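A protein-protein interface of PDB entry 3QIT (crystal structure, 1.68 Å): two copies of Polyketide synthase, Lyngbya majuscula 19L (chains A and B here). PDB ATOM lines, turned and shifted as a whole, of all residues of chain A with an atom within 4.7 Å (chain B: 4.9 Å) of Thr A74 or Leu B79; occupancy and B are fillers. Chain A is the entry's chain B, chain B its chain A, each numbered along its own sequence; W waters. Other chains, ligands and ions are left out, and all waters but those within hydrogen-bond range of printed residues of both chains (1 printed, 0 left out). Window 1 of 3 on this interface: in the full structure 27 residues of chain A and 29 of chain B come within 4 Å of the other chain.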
ATOM      1  N   MET A  72     -31.952  12.057 -14.651  1.00  0.00           N
ATOM      2  CA  MET A  72     -30.767  11.233 -14.408  1.00  0.00           C
ATOM      3  C   MET A  72     -31.060   9.778 -14.740  1.00  0.00           C
ATOM      4  O   MET A  72     -31.875   9.132 -14.073  1.00  0.00           O
ATOM      5  CB  MET A  72     -30.278  11.353 -12.995  1.00  0.00           C
ATOM      6  CG  MET A  72     -28.856  10.741 -12.884  1.00  0.00           C
ATOM      7  SD  MET A  72     -28.057  11.384 -11.490  1.00  0.00           S
ATOM      8  CE  MET A  72     -29.236  10.922 -10.230  1.00  0.00           C
ATOM      9  N   VAL A  73     -30.359   9.274 -15.752  1.00  0.00           N
ATOM     10  CA  VAL A  73     -30.637   7.940 -16.351  1.00  0.00           C
ATOM     11  C   VAL A  73     -30.619   6.788 -15.348  1.00  0.00           C
ATOM     12  O   VAL A  73     -31.365   5.817 -15.500  1.00  0.00           O
ATOM     13  CB  VAL A  73     -29.582   7.595 -17.454  1.00  0.00           C
ATOM     14  CG1 VAL A  73     -29.880   6.220 -18.066  1.00  0.00           C
ATOM     15  CG2 VAL A  73     -29.570   8.648 -18.529  1.00  0.00           C
ATOM     16  N   THR A  74     -29.753   6.895 -14.342  1.00  0.00           N
ATOM     17  CA  THR A  74     -29.630   5.857 -13.313  1.00  0.00           C
ATOM     18  C   THR A  74     -30.866   5.738 -12.425  1.00  0.00           C
ATOM     19  O   THR A  74     -30.996   4.794 -11.642  1.00  0.00           O
ATOM     20  CB  THR A  74     -28.391   6.060 -12.423  1.00  0.00           C
ATOM     21  OG1 THR A  74     -28.401   7.376 -11.861  1.00  0.00           O
ATOM     22  CG2 THR A  74     -27.125   5.838 -13.220  1.00  0.00           C
ATOM     23  N   SER A  75     -31.772   6.692 -12.574  1.00  0.00           N
ATOM     24  CA  SER A  75     -33.049   6.702 -11.842  1.00  0.00           C
ATOM     25  C   SER A  75     -34.005   5.643 -12.371  1.00  0.00           C
ATOM     26  O   SER A  75     -34.934   5.239 -11.659  1.00  0.00           O
ATOM     27  CB  SER A  75     -33.702   8.094 -11.899  1.00  0.00           C
ATOM     28  OG  SER A  75     -32.875   9.069 -11.258  1.00  0.00           O
ATOM     29  N   TYR A  76     -33.809   5.210 -13.619  1.00  0.00           N
ATOM     30  CA  TYR A  76     -34.661   4.162 -14.199  1.00  0.00           C
ATOM     31  C   TYR A  76     -34.237   2.807 -13.648  1.00  0.00           C
ATOM     32  O   TYR A  76     -33.153   2.284 -13.970  1.00  0.00           O
ATOM     33  CB  TYR A  76     -34.574   4.164 -15.731  1.00  0.00           C
ATOM     34  CG  TYR A  76     -35.265   5.332 -16.396  1.00  0.00           C
ATOM     35  CD1 TYR A  76     -36.652   5.452 -16.374  1.00  0.00           C
ATOM     36  CD2 TYR A  76     -34.530   6.317 -17.053  1.00  0.00           C
ATOM     37  CE1 TYR A  76     -37.288   6.524 -16.995  1.00  0.00           C
ATOM     38  CE2 TYR A  76     -35.155   7.415 -17.668  1.00  0.00           C
ATOM     39  CZ  TYR A  76     -36.521   7.514 -17.623  1.00  0.00           C
ATOM     40  OH  TYR A  76     -37.100   8.582 -18.275  1.00  0.00           O
ATOM     41  N   LEU A 144     -21.077  -4.032 -15.956  1.00  0.00           N
ATOM     42  CA  LEU A 144     -21.032  -2.666 -15.459  1.00  0.00           C
ATOM     43  C   LEU A 144     -20.428  -1.716 -16.497  1.00  0.00           C
ATOM     44  O   LEU A 144     -20.881  -0.581 -16.642  1.00  0.00           O
ATOM     45  CB  LEU A 144     -20.266  -2.574 -14.138  1.00  0.00           C
ATOM     46  CG  LEU A 144     -20.208  -1.181 -13.507  1.00  0.00           C
ATOM     47  CD1 LEU A 144     -21.628  -0.682 -13.190  1.00  0.00           C
ATOM     48  CD2 LEU A 144     -19.386  -1.268 -12.253  1.00  0.00           C
ATOM     49  N   CYS A 147     -23.019  -1.037 -19.054  1.00  0.00           N
ATOM     50  CA  CYS A 147     -24.047  -0.209 -18.429  1.00  0.00           C
ATOM     51  C   CYS A 147     -23.622   1.267 -18.302  1.00  0.00           C
ATOM     52  O   CYS A 147     -24.370   2.170 -18.703  1.00  0.00           O
ATOM     53  CB  CYS A 147     -24.402  -0.772 -17.065  1.00  0.00           C
ATOM     54  SG  CYS A 147     -25.611   0.278 -16.201  1.00  0.00           S
ATOM     55  N   LEU A 148     -22.412   1.506 -17.794  1.00  0.00           N
ATOM     56  CA  LEU A 148     -21.892   2.870 -17.632  1.00  0.00           C
ATOM     57  C   LEU A 148     -21.732   3.580 -18.971  1.00  0.00           C
ATOM     58  O   LEU A 148     -22.016   4.777 -19.096  1.00  0.00           O
ATOM     59  CB  LEU A 148     -20.565   2.876 -16.872  1.00  0.00           C
ATOM     60  CG  LEU A 148     -20.661   3.148 -15.372  1.00  0.00           C
ATOM     61  CD1 LEU A 148     -21.529   2.105 -14.719  1.00  0.00           C
ATOM     62  CD2 LEU A 148     -19.275   3.182 -14.742  1.00  0.00           C
ATOM     63  N   LEU A 151     -25.394   4.375 -20.076  1.00  0.00           N
ATOM     64  CA  LEU A 151     -25.910   5.484 -19.252  1.00  0.00           C
ATOM     65  C   LEU A 151     -25.429   6.861 -19.728  1.00  0.00           C
ATOM     66  O   LEU A 151     -26.129   7.874 -19.536  1.00  0.00           O
ATOM     67  CB  LEU A 151     -25.502   5.297 -17.786  1.00  0.00           C
ATOM     68  CG  LEU A 151     -26.010   4.126 -16.935  1.00  0.00           C
ATOM     69  CD1 LEU A 151     -25.186   4.063 -15.667  1.00  0.00           C
ATOM     70  CD2 LEU A 151     -27.477   4.243 -16.585  1.00  0.00           C
ATOM     71  N   SER B  75     -33.262   7.385  -6.616  1.00  0.00           N
ATOM     72  CA  SER B  75     -32.069   7.755  -7.382  1.00  0.00           C
ATOM     73  C   SER B  75     -30.777   7.544  -6.594  1.00  0.00           C
ATOM     74  O   SER B  75     -29.699   7.502  -7.175  1.00  0.00           O
ATOM     75  CB  SER B  75     -32.141   9.200  -7.884  1.00  0.00           C
ATOM     76  OG  SER B  75     -33.329   9.410  -8.637  1.00  0.00           O
ATOM     77  N   SER B  77     -28.225   5.435  -5.235  1.00  0.00           N
ATOM     78  CA  SER B  77     -27.755   4.052  -5.444  1.00  0.00           C
ATOM     79  C   SER B  77     -26.261   4.119  -5.725  1.00  0.00           C
ATOM     80  O   SER B  77     -25.745   5.164  -6.136  1.00  0.00           O
ATOM     81  CB  SER B  77     -28.466   3.401  -6.643  1.00  0.00           C
ATOM     82  OG  SER B  77     -28.141   4.090  -7.867  1.00  0.00           O
ATOM     83  N   SER B  78     -25.563   3.001  -5.543  1.00  0.00           N
ATOM     84  CA  SER B  78     -24.159   2.954  -5.904  1.00  0.00           C
ATOM     85  C   SER B  78     -23.987   3.201  -7.400  1.00  0.00           C
ATOM     86  O   SER B  78     -23.013   3.818  -7.811  1.00  0.00           O
ATOM     87  CB  SER B  78     -23.538   1.623  -5.490  1.00  0.00           C
ATOM     88  OG  SER B  78     -23.681   1.432  -4.093  1.00  0.00           O
ATOM     89  N   LEU B  79     -24.954   2.731  -8.210  1.00  0.00           N
ATOM     90  CA  LEU B  79     -24.908   2.979  -9.663  1.00  0.00           C
ATOM     91  C   LEU B  79     -24.917   4.471  -9.987  1.00  0.00           C
ATOM     92  O   LEU B  79     -24.147   4.928 -10.829  1.00  0.00           O
ATOM     93  CB  LEU B  79     -26.057   2.277 -10.402  1.00  0.00           C
ATOM     94  CG  LEU B  79     -26.038   2.479 -11.928  1.00  0.00           C
ATOM     95  CD1 LEU B  79     -24.831   1.765 -12.494  1.00  0.00           C
ATOM     96  CD2 LEU B  79     -27.302   1.941 -12.590  1.00  0.00           C
ATOM     97  N   THR B  80     -25.803   5.224  -9.329  1.00  0.00           N
ATOM     98  CA  THR B  80     -25.816   6.688  -9.489  1.00  0.00           C
ATOM     99  C   THR B  80     -24.469   7.321  -9.103  1.00  0.00           C
ATOM    100  O   THR B  80     -23.928   8.130  -9.847  1.00  0.00           O
ATOM    101  CB  THR B  80     -26.968   7.304  -8.702  1.00  0.00           C
ATOM    102  OG1 THR B  80     -28.209   6.912  -9.309  1.00  0.00           O
ATOM    103  CG2 THR B  80     -26.848   8.833  -8.669  1.00  0.00           C
ATOM    104  N   PHE B  81     -23.894   6.927  -7.963  1.00  0.00           N
ATOM    105  CA  PHE B  81     -22.569   7.454  -7.570  1.00  0.00           C
ATOM    106  C   PHE B  81     -21.478   7.078  -8.558  1.00  0.00           C
ATOM    107  O   PHE B  81     -20.570   7.866  -8.786  1.00  0.00           O
ATOM    108  CB  PHE B  81     -22.180   6.968  -6.171  1.00  0.00           C
ATOM    109  CG  PHE B  81     -23.058   7.516  -5.055  1.00  0.00           C
ATOM    110  CD1 PHE B  81     -23.531   8.836  -5.088  1.00  0.00           C
ATOM    111  CD2 PHE B  81     -23.330   6.739  -3.942  1.00  0.00           C
ATOM    112  CE1 PHE B  81     -24.331   9.359  -4.034  1.00  0.00           C
ATOM    113  CE2 PHE B  81     -24.129   7.228  -2.887  1.00  0.00           C
ATOM    114  CZ  PHE B  81     -24.630   8.551  -2.933  1.00  0.00           C
ATOM    115  N   LEU B  82     -21.562   5.876  -9.139  1.00  0.00           N
ATOM    116  CA  LEU B  82     -20.555   5.453 -10.114  1.00  0.00           C
ATOM    117  C   LEU B  82     -20.682   6.274 -11.403  1.00  0.00           C
ATOM    118  O   LEU B  82     -19.696   6.734 -11.966  1.00  0.00           O
ATOM    119  CB  LEU B  82     -20.709   3.956 -10.413  1.00  0.00           C
ATOM    120  CG  LEU B  82     -20.304   2.998  -9.281  1.00  0.00           C
ATOM    121  CD1 LEU B  82     -20.631   1.601  -9.781  1.00  0.00           C
ATOM    122  CD2 LEU B  82     -18.783   3.146  -9.028  1.00  0.00           C
ATOM    123  N   ALA B  83     -21.912   6.526 -11.825  1.00  0.00           N
ATOM    124  CA  ALA B  83     -22.124   7.364 -13.003  1.00  0.00           C
ATOM    125  C   ALA B  83     -21.622   8.794 -12.740  1.00  0.00           C
ATOM    126  O   ALA B  83     -21.143   9.473 -13.652  1.00  0.00           O
ATOM    127  CB  ALA B  83     -23.616   7.396 -13.388  1.00  0.00           C
ATOM    128  N   PRO B 217     -23.874  -2.333  -7.754  1.00  0.00           N
ATOM    129  CA  PRO B 217     -25.102  -2.618  -8.497  1.00  0.00           C
ATOM    130  C   PRO B 217     -25.368  -4.113  -8.676  1.00  0.00           C
ATOM    131  O   PRO B 217     -26.533  -4.535  -8.730  1.00  0.00           O
ATOM    132  CB  PRO B 217     -24.850  -1.958  -9.851  1.00  0.00           C
ATOM    133  CG  PRO B 217     -23.930  -0.809  -9.531  1.00  0.00           C
ATOM    134  CD  PRO B 217     -23.025  -1.347  -8.459  1.00  0.00           C
HETATM  135  O   HOH W   1     -30.239   3.574  -9.554  1.00  0.00           O
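The side-chain hydroxyl (OG) of Ser B75 lies within hydrogen-bond range of the side-chain hydroxyl (OG) of Ser A75, at 2.7 Å.
The side-chain hydroxyl of Thr A74 is in hydrogen-bond range of the side-chain hydroxyl of Thr B80, at 2.6 Å.
O of Ser B75 is in hydrogen-bond range of OG1 of Thr B80 (2.7 Å).
OG of Ser B77 lies within hydrogen-bond range of N of Thr B80 (3.0 Å).
The side-chain hydroxyl (OG) of Ser B77 lies close to the backbone NH (N) of Leu B79 (3.5 Å).
O of Met A72 is in hydrogen-bond range of OG of Ser A75 (3.0 Å).
Met A72 touches Thr B80.
Leu B79 touches Thr A74.
Thr A74 touches Ala B83.
CD1 of Leu B82 touches CD2 of Leu A144, at 3.99 Å.
CD1 of Leu A148 touches CD1 of Leu B79 (3.996 Å).
Leu A151 touches Leu B79.
Thr A74 touches just these residues of chain B: Leu B79, Thr B80 and Ala B83.
Of the printed residues of chain B, Ser A75 touches Ser B75 (2.7 Å).
Tyr A76 touches none of the printed residues of chain B.
Of the printed residues of chain B, Leu A144 touches Leu B82 (3.99 Å).
Of the printed residues of chain B, Leu A151 touches Leu B79.
Of the printed residues of chain A, Leu B79 touches Thr A74, Leu A148 and Leu A151.
Of the printed residues of chain A, Thr B80 touches Met A72 (3.5 Å) and Thr A74 (2.6 Å).
Phe B81 touches none of the printed residues of chain A.
The nearest residue of chain B that does not touch Thr A74 is Ser B77 (4.8 Å).
The nearest printed residue of chain A that does not touch Leu B79 is Cys A147 (4.1 Å).
Hydrophobic or aromatic side chains of chain A within 4 Å of the printed part of chain B: Met A72, Leu A144, Leu A148 and Leu A151.
Of the 9 printed residues of chain B, 5 touch a printed residue of chain A.
Printed residues of chain B that touch a printed residue of chain A: Ser B75, Leu B79, Thr B80, Leu B82 and Ala B83.
Among the printed residues, no Asp or Glu carboxylate lies within 4 Å of a Lys or Arg side-chain nitrogen of the other chain.
Ser B75 touches its own counterpart, Ser A75.
Position printed for both chains: 75.
Of the 8 pairs that touch across the chains among the printed residues, 1 has its exchanged pair printed and touching as well.
Water W1 bridges the backbone carbonyl oxygen (O) of Thr A74 and the side-chain hydroxyl (OG) of Ser B77.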
